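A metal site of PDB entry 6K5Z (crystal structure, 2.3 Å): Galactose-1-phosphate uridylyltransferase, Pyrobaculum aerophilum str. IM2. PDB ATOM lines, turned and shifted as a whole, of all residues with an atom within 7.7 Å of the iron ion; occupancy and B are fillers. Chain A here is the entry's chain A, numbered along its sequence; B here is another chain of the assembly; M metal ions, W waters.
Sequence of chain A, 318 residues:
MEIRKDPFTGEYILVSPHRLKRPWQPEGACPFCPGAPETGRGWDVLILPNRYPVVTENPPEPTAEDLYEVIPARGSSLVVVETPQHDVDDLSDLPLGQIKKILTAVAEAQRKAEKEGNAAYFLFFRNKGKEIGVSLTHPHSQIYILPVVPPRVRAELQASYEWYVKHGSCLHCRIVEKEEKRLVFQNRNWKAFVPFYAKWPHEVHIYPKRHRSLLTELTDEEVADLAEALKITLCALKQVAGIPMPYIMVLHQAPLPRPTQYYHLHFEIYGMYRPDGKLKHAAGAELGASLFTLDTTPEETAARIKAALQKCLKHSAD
The iron ion is bound by the side-chain carboxylate (OE2) of Glu 156 (2.2 Å), the side-chain carboxylate (OE2) of Glu 268 (2.2 Å), a ring nitrogen (NE2) of His 266 (2.3 Å), a ring nitrogen (ND1) of His 252 (2.3 Å), water W1 (2.4 Å) and the side-chain carboxylate (OE1) of Glu 156 (2.5 Å).
The side-chain hydroxyl (OH) of Tyr 207 is in hydrogen-bond range of a ring nitrogen (ND1) of His 266, 3.3 Å away.
OE1 of Glu 268 sits at hydrogen-bond distance from OH of Tyr 270 (2.6 Å).
NE2 of His 252 sits at hydrogen-bond distance from O of Gly 288 of chain B.
The side-chain carboxylate (OE2) of Glu 268 sits close to a ring nitrogen (ND1) of His 205, 3.4 Å away.
The side-chain hydroxyl of Tyr 263 lies close to the side-chain carboxylate of Glu 156 (2.6 Å).
N of Glu 268 lies within hydrogen-bond range of O of Val 250 (2.8 Å).
A ring nitrogen (ND1) of His 266 lies within hydrogen-bond range of the backbone carbonyl oxygen of His 264.
Four residues have an atom within 4 Å of the iron ion: Glu 156, His 252, His 266 and Glu 268.
The nearest printed residue that does not touch the iron ion is Tyr 263 (4.3 Å).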
ATOM      1  N   ARG A 152     -20.207  10.396   6.986  1.00  0.00           N
ATOM      2  CA  ARG A 152     -21.090  11.531   7.304  1.00  0.00           C
ATOM      3  C   ARG A 152     -22.353  11.441   6.467  1.00  0.00           C
ATOM      4  O   ARG A 152     -23.428  11.767   6.957  1.00  0.00           O
ATOM      5  CB  ARG A 152     -20.384  12.877   7.048  1.00  0.00           C
ATOM      6  CG  ARG A 152     -21.274  14.109   7.141  1.00  0.00           C
ATOM      7  CD  ARG A 152     -20.418  15.343   7.226  1.00  0.00           C
ATOM      8  NE  ARG A 152     -19.915  15.510   8.575  1.00  0.00           N
ATOM      9  CZ  ARG A 152     -20.456  16.290   9.522  1.00  0.00           C
ATOM     10  NH1 ARG A 152     -21.517  17.062   9.286  1.00  0.00           N
ATOM     11  NH2 ARG A 152     -19.893  16.299  10.731  1.00  0.00           N
ATOM     12  N   VAL A 153     -22.211  11.064   5.206  1.00  0.00           N
ATOM     13  CA  VAL A 153     -23.354  10.886   4.315  1.00  0.00           C
ATOM     14  C   VAL A 153     -24.233   9.692   4.770  1.00  0.00           C
ATOM     15  O   VAL A 153     -25.463   9.817   4.778  1.00  0.00           O
ATOM     16  CB  VAL A 153     -22.910  10.732   2.841  1.00  0.00           C
ATOM     17  CG1 VAL A 153     -24.103  10.378   1.978  1.00  0.00           C
ATOM     18  CG2 VAL A 153     -22.302  12.009   2.305  1.00  0.00           C
ATOM     19  N   GLU A 156     -26.359  10.818   7.581  1.00  0.00           N
ATOM     20  CA  GLU A 156     -27.485  11.712   7.124  1.00  0.00           C
ATOM     21  C   GLU A 156     -28.610  10.919   6.485  1.00  0.00           C
ATOM     22  O   GLU A 156     -29.763  11.327   6.586  1.00  0.00           O
ATOM     23  CB  GLU A 156     -27.015  12.747   6.103  1.00  0.00           C
ATOM     24  CG  GLU A 156     -26.058  13.780   6.657  1.00  0.00           C
ATOM     25  CD  GLU A 156     -25.936  14.980   5.773  1.00  0.00           C
ATOM     26  OE1 GLU A 156     -26.515  14.968   4.637  1.00  0.00           O
ATOM     27  OE2 GLU A 156     -25.291  15.925   6.253  1.00  0.00           O
ATOM     28  N   HIS A 172     -35.834  17.009   4.311  1.00  0.00           N
ATOM     29  CA  HIS A 172     -35.169  18.027   3.511  1.00  0.00           C
ATOM     30  C   HIS A 172     -36.167  18.859   2.707  1.00  0.00           C
ATOM     31  O   HIS A 172     -36.043  20.079   2.658  1.00  0.00           O
ATOM     32  CB  HIS A 172     -34.186  17.394   2.536  1.00  0.00           C
ATOM     33  CG  HIS A 172     -33.155  16.529   3.190  1.00  0.00           C
ATOM     34  ND1 HIS A 172     -31.905  16.996   3.528  1.00  0.00           N
ATOM     35  CD2 HIS A 172     -33.184  15.230   3.554  1.00  0.00           C
ATOM     36  CE1 HIS A 172     -31.208  16.017   4.080  1.00  0.00           C
ATOM     37  NE2 HIS A 172     -31.963  14.935   4.105  1.00  0.00           N
ATOM     38  N   TYR A 197     -28.872  24.579  11.926  1.00  0.00           N
ATOM     39  CA  TYR A 197     -27.892  23.690  12.559  1.00  0.00           C
ATOM     40  C   TYR A 197     -26.443  23.932  12.000  1.00  0.00           C
ATOM     41  O   TYR A 197     -25.574  23.050  12.070  1.00  0.00           O
ATOM     42  CB  TYR A 197     -28.338  22.232  12.370  1.00  0.00           C
ATOM     43  CG  TYR A 197     -28.862  21.930  10.971  1.00  0.00           C
ATOM     44  CD1 TYR A 197     -30.173  22.291  10.584  1.00  0.00           C
ATOM     45  CD2 TYR A 197     -28.054  21.284  10.019  1.00  0.00           C
ATOM     46  CE1 TYR A 197     -30.646  22.054   9.291  1.00  0.00           C
ATOM     47  CE2 TYR A 197     -28.530  21.015   8.752  1.00  0.00           C
ATOM     48  CZ  TYR A 197     -29.816  21.409   8.385  1.00  0.00           C
ATOM     49  OH  TYR A 197     -30.262  21.142   7.127  1.00  0.00           O
ATOM     50  N   GLU A 203     -21.536  29.000   6.891  1.00  0.00           N
ATOM     51  CA  GLU A 203     -22.103  27.793   6.282  1.00  0.00           C
ATOM     52  C   GLU A 203     -23.329  28.099   5.450  1.00  0.00           C
ATOM     53  O   GLU A 203     -24.233  28.773   5.926  1.00  0.00           O
ATOM     54  CB  GLU A 203     -22.439  26.805   7.377  1.00  0.00           C
ATOM     55  CG  GLU A 203     -22.946  25.460   6.855  1.00  0.00           C
ATOM     56  CD  GLU A 203     -22.632  24.300   7.767  1.00  0.00           C
ATOM     57  OE1 GLU A 203     -21.946  24.484   8.794  1.00  0.00           O
ATOM     58  OE2 GLU A 203     -23.014  23.179   7.421  1.00  0.00           O
ATOM     59  N   HIS A 205     -26.027  25.984   2.713  1.00  0.00           N
ATOM     60  CA  HIS A 205     -26.432  24.773   1.985  1.00  0.00           C
ATOM     61  C   HIS A 205     -27.269  25.183   0.811  1.00  0.00           C
ATOM     62  O   HIS A 205     -28.041  26.159   0.896  1.00  0.00           O
ATOM     63  CB  HIS A 205     -27.172  23.778   2.863  1.00  0.00           C
ATOM     64  CG  HIS A 205     -26.339  23.240   3.997  1.00  0.00           C
ATOM     65  ND1 HIS A 205     -26.771  22.209   4.794  1.00  0.00           N
ATOM     66  CD2 HIS A 205     -25.130  23.602   4.476  1.00  0.00           C
ATOM     67  CE1 HIS A 205     -25.869  21.955   5.729  1.00  0.00           C
ATOM     68  NE2 HIS A 205     -24.860  22.787   5.553  1.00  0.00           N
ATOM     69  N   TYR A 207     -29.830  23.706  -1.974  1.00  0.00           N
ATOM     70  CA  TYR A 207     -30.789  22.591  -2.187  1.00  0.00           C
ATOM     71  C   TYR A 207     -31.607  22.854  -3.411  1.00  0.00           C
ATOM     72  O   TYR A 207     -31.980  24.010  -3.668  1.00  0.00           O
ATOM     73  CB  TYR A 207     -31.767  22.541  -1.045  1.00  0.00           C
ATOM     74  CG  TYR A 207     -31.365  21.655   0.075  1.00  0.00           C
ATOM     75  CD1 TYR A 207     -31.681  20.322   0.047  1.00  0.00           C
ATOM     76  CD2 TYR A 207     -30.736  22.171   1.188  1.00  0.00           C
ATOM     77  CE1 TYR A 207     -31.338  19.504   1.101  1.00  0.00           C
ATOM     78  CE2 TYR A 207     -30.353  21.364   2.248  1.00  0.00           C
ATOM     79  CZ  TYR A 207     -30.665  20.043   2.206  1.00  0.00           C
ATOM     80  OH  TYR A 207     -30.328  19.255   3.229  1.00  0.00           O
ATOM     81  N   VAL A 250     -18.920  20.501  -0.408  1.00  0.00           N
ATOM     82  CA  VAL A 250     -19.157  19.092  -0.662  1.00  0.00           C
ATOM     83  C   VAL A 250     -20.593  18.856  -1.135  1.00  0.00           C
ATOM     84  O   VAL A 250     -21.537  19.497  -0.671  1.00  0.00           O
ATOM     85  CB  VAL A 250     -18.838  18.291   0.598  1.00  0.00           C
ATOM     86  CG1 VAL A 250     -19.695  18.736   1.768  1.00  0.00           C
ATOM     87  CG2 VAL A 250     -18.984  16.818   0.329  1.00  0.00           C
ATOM     88  N   LEU A 251     -20.746  17.946  -2.079  1.00  0.00           N
ATOM     89  CA  LEU A 251     -22.051  17.493  -2.565  1.00  0.00           C
ATOM     90  C   LEU A 251     -22.504  16.237  -1.826  1.00  0.00           C
ATOM     91  O   LEU A 251     -21.895  15.171  -1.948  1.00  0.00           O
ATOM     92  CB  LEU A 251     -21.999  17.206  -4.066  1.00  0.00           C
ATOM     93  CG  LEU A 251     -23.255  16.558  -4.712  1.00  0.00           C
ATOM     94  CD1 LEU A 251     -24.445  17.480  -4.569  1.00  0.00           C
ATOM     95  CD2 LEU A 251     -22.958  16.270  -6.202  1.00  0.00           C
ATOM     96  N   HIS A 252     -23.564  16.397  -1.060  1.00  0.00           N
ATOM     97  CA  HIS A 252     -24.219  15.321  -0.372  1.00  0.00           C
ATOM     98  C   HIS A 252     -25.369  14.867  -1.227  1.00  0.00           C
ATOM     99  O   HIS A 252     -26.330  15.623  -1.437  1.00  0.00           O
ATOM    100  CB  HIS A 252     -24.735  15.828   0.965  1.00  0.00           C
ATOM    101  CG  HIS A 252     -23.656  16.013   1.990  1.00  0.00           C
ATOM    102  ND1 HIS A 252     -23.923  16.397   3.277  1.00  0.00           N
ATOM    103  CD2 HIS A 252     -22.317  15.836   1.903  1.00  0.00           C
ATOM    104  CE1 HIS A 252     -22.786  16.509   3.940  1.00  0.00           C
ATOM    105  NE2 HIS A 252     -21.800  16.164   3.123  1.00  0.00           N
ATOM    106  N   GLN A 253     -25.234  13.673  -1.775  1.00  0.00           N
ATOM    107  CA  GLN A 253     -26.269  13.043  -2.573  1.00  0.00           C
ATOM    108  C   GLN A 253     -26.383  11.549  -2.191  1.00  0.00           C
ATOM    109  O   GLN A 253     -25.615  11.019  -1.358  1.00  0.00           O
ATOM    110  CB  GLN A 253     -25.957  13.243  -4.056  1.00  0.00           C
ATOM    111  CG  GLN A 253     -24.788  12.424  -4.555  1.00  0.00           C
ATOM    112  CD  GLN A 253     -24.559  12.596  -6.042  1.00  0.00           C
ATOM    113  OE1 GLN A 253     -25.512  12.547  -6.818  1.00  0.00           O
ATOM    114  NE2 GLN A 253     -23.278  12.750  -6.454  1.00  0.00           N
ATOM    115  N   TYR A 263     -34.028  10.905   0.899  1.00  0.00           N
ATOM    116  CA  TYR A 263     -32.842  11.758   0.864  1.00  0.00           C
ATOM    117  C   TYR A 263     -32.905  12.683  -0.332  1.00  0.00           C
ATOM    118  O   TYR A 263     -33.465  12.359  -1.390  1.00  0.00           O
ATOM    119  CB  TYR A 263     -31.548  10.931   0.840  1.00  0.00           C
ATOM    120  CG  TYR A 263     -30.307  11.692   1.245  1.00  0.00           C
ATOM    121  CD1 TYR A 263     -30.215  12.269   2.493  1.00  0.00           C
ATOM    122  CD2 TYR A 263     -29.221  11.800   0.390  1.00  0.00           C
ATOM    123  CE1 TYR A 263     -29.079  12.938   2.888  1.00  0.00           C
ATOM    124  CE2 TYR A 263     -28.071  12.510   0.755  1.00  0.00           C
ATOM    125  CZ  TYR A 263     -28.000  13.069   2.009  1.00  0.00           C
ATOM    126  OH  TYR A 263     -26.881  13.753   2.425  1.00  0.00           O
ATOM    127  N   HIS A 264     -32.282  13.836  -0.162  1.00  0.00           N
ATOM    128  CA  HIS A 264     -32.481  14.962  -1.044  1.00  0.00           C
ATOM    129  C   HIS A 264     -31.124  15.629  -1.161  1.00  0.00           C
ATOM    130  O   HIS A 264     -30.574  16.108  -0.164  1.00  0.00           O
ATOM    131  CB  HIS A 264     -33.549  15.863  -0.412  1.00  0.00           C
ATOM    132  CG  HIS A 264     -33.940  17.084  -1.201  1.00  0.00           C
ATOM    133  ND1 HIS A 264     -35.211  17.637  -1.131  1.00  0.00           N
ATOM    134  CD2 HIS A 264     -33.227  17.904  -2.006  1.00  0.00           C
ATOM    135  CE1 HIS A 264     -35.260  18.719  -1.866  1.00  0.00           C
ATOM    136  NE2 HIS A 264     -34.071  18.910  -2.416  1.00  0.00           N
ATOM    137  N   LEU A 265     -30.586  15.650  -2.375  1.00  0.00           N
ATOM    138  CA  LEU A 265     -29.255  16.121  -2.580  1.00  0.00           C
ATOM    139  C   LEU A 265     -29.045  17.607  -2.218  1.00  0.00           C
ATOM    140  O   LEU A 265     -29.957  18.450  -2.424  1.00  0.00           O
ATOM    141  CB  LEU A 265     -28.797  15.850  -4.028  1.00  0.00           C
ATOM    142  CG  LEU A 265     -29.198  16.786  -5.159  1.00  0.00           C
ATOM    143  CD1 LEU A 265     -28.321  18.041  -5.301  1.00  0.00           C
ATOM    144  CD2 LEU A 265     -29.176  15.988  -6.453  1.00  0.00           C
ATOM    145  N   HIS A 266     -27.842  17.927  -1.723  1.00  0.00           N
ATOM    146  CA  HIS A 266     -27.478  19.316  -1.492  1.00  0.00           C
ATOM    147  C   HIS A 266     -25.983  19.534  -1.466  1.00  0.00           C
ATOM    148  O   HIS A 266     -25.225  18.584  -1.217  1.00  0.00           O
ATOM    149  CB  HIS A 266     -28.094  19.816  -0.187  1.00  0.00           C
ATOM    150  CG  HIS A 266     -27.789  18.928   0.958  1.00  0.00           C
ATOM    151  ND1 HIS A 266     -28.360  17.678   1.103  1.00  0.00           N
ATOM    152  CD2 HIS A 266     -26.943  19.077   1.998  1.00  0.00           C
ATOM    153  CE1 HIS A 266     -27.866  17.101   2.183  1.00  0.00           C
ATOM    154  NE2 HIS A 266     -27.005  17.927   2.741  1.00  0.00           N
ATOM    155  N   PHE A 267     -25.587  20.794  -1.689  1.00  0.00           N
ATOM    156  CA  PHE A 267     -24.191  21.187  -1.571  1.00  0.00           C
ATOM    157  C   PHE A 267     -24.034  21.850  -0.236  1.00  0.00           C
ATOM    158  O   PHE A 267     -24.840  22.670   0.056  1.00  0.00           O
ATOM    159  CB  PHE A 267     -23.857  22.192  -2.652  1.00  0.00           C
ATOM    160  CG  PHE A 267     -23.782  21.604  -4.024  1.00  0.00           C
ATOM    161  CD1 PHE A 267     -24.911  21.449  -4.761  1.00  0.00           C
ATOM    162  CD2 PHE A 267     -22.585  21.220  -4.569  1.00  0.00           C
ATOM    163  CE1 PHE A 267     -24.866  20.928  -6.033  1.00  0.00           C
ATOM    164  CE2 PHE A 267     -22.501  20.705  -5.852  1.00  0.00           C
ATOM    165  CZ  PHE A 267     -23.645  20.548  -6.581  1.00  0.00           C
ATOM    166  N   GLU A 268     -23.052  21.478   0.585  1.00  0.00           N
ATOM    167  CA  GLU A 268     -22.726  22.253   1.779  1.00  0.00           C
ATOM    168  C   GLU A 268     -21.459  23.079   1.572  1.00  0.00           C
ATOM    169  O   GLU A 268     -20.512  22.564   1.066  1.00  0.00           O
ATOM    170  CB  GLU A 268     -22.526  21.315   2.974  1.00  0.00           C
ATOM    171  CG  GLU A 268     -23.654  20.294   3.098  1.00  0.00           C
ATOM    172  CD  GLU A 268     -23.805  19.674   4.489  1.00  0.00           C
ATOM    173  OE1 GLU A 268     -22.785  19.465   5.202  1.00  0.00           O
ATOM    174  OE2 GLU A 268     -24.966  19.382   4.858  1.00  0.00           O
ATOM    175  N   TYR A 270     -18.629  25.380   3.599  1.00  0.00           N
ATOM    176  CA  TYR A 270     -18.094  25.811   4.895  1.00  0.00           C
ATOM    177  C   TYR A 270     -17.044  26.890   4.681  1.00  0.00           C
ATOM    178  O   TYR A 270     -15.920  26.600   4.339  1.00  0.00           O
ATOM    179  CB  TYR A 270     -17.463  24.644   5.646  1.00  0.00           C
ATOM    180  CG  TYR A 270     -18.231  23.338   5.642  1.00  0.00           C
ATOM    181  CD1 TYR A 270     -19.615  23.305   5.664  1.00  0.00           C
ATOM    182  CD2 TYR A 270     -17.556  22.130   5.751  1.00  0.00           C
ATOM    183  CE1 TYR A 270     -20.307  22.096   5.720  1.00  0.00           C
ATOM    184  CE2 TYR A 270     -18.243  20.937   5.809  1.00  0.00           C
ATOM    185  CZ  TYR A 270     -19.624  20.936   5.805  1.00  0.00           C
ATOM    186  OH  TYR A 270     -20.326  19.742   5.870  1.00  0.00           O
ATOM    187  N   ASP B   6     -28.238  19.045  15.059  1.00  0.00           N
ATOM    188  CA  ASP B   6     -28.273  18.810  13.618  1.00  0.00           C
ATOM    189  C   ASP B   6     -29.137  17.552  13.431  1.00  0.00           C
ATOM    190  O   ASP B   6     -28.803  16.457  13.939  1.00  0.00           O
ATOM    191  CB  ASP B   6     -26.827  18.668  13.073  1.00  0.00           C
ATOM    192  CG  ASP B   6     -26.743  18.341  11.561  1.00  0.00           C
ATOM    193  OD1 ASP B   6     -27.491  17.471  11.089  1.00  0.00           O
ATOM    194  OD2 ASP B   6     -25.840  18.894  10.864  1.00  0.00           O
ATOM    195  N   PHE B   8     -29.767  15.723  10.898  1.00  0.00           N
ATOM    196  CA  PHE B   8     -29.185  14.651  10.066  1.00  0.00           C
ATOM    197  C   PHE B   8     -27.997  13.906  10.661  1.00  0.00           C
ATOM    198  O   PHE B   8     -27.797  12.747  10.343  1.00  0.00           O
ATOM    199  CB  PHE B   8     -28.857  15.201   8.677  1.00  0.00           C
ATOM    200  CG  PHE B   8     -30.036  15.816   8.017  1.00  0.00           C
ATOM    201  CD1 PHE B   8     -31.083  15.006   7.596  1.00  0.00           C
ATOM    202  CD2 PHE B   8     -30.148  17.203   7.898  1.00  0.00           C
ATOM    203  CE1 PHE B   8     -32.214  15.584   7.024  1.00  0.00           C
ATOM    204  CE2 PHE B   8     -31.262  17.787   7.336  1.00  0.00           C
ATOM    205  CZ  PHE B   8     -32.309  16.980   6.890  1.00  0.00           C
ATOM    206  N   THR B   9     -27.206  14.581  11.485  1.00  0.00           N
ATOM    207  CA  THR B   9     -26.002  13.976  12.093  1.00  0.00           C
ATOM    208  C   THR B   9     -26.144  13.727  13.580  1.00  0.00           C
ATOM    209  O   THR B   9     -25.457  12.879  14.132  1.00  0.00           O
ATOM    210  CB  THR B   9     -24.780  14.872  11.879  1.00  0.00           C
ATOM    211  OG1 THR B   9     -25.038  16.147  12.448  1.00  0.00           O
ATOM    212  CG2 THR B   9     -24.487  15.060  10.395  1.00  0.00           C
ATOM    213  N   GLY B 288     -16.334  17.328   5.444  1.00  0.00           N
ATOM    214  CA  GLY B 288     -17.464  17.239   4.537  1.00  0.00           C
ATOM    215  C   GLY B 288     -18.091  15.885   4.438  1.00  0.00           C
ATOM    216  O   GLY B 288     -19.319  15.764   4.230  1.00  0.00           O
HETATM  217 FE    FE M   1     -25.685  17.282   4.533  1.00  0.00          FE
HETATM  218  O   HOH W   1     -27.344  18.348   5.965  1.00  0.00           O
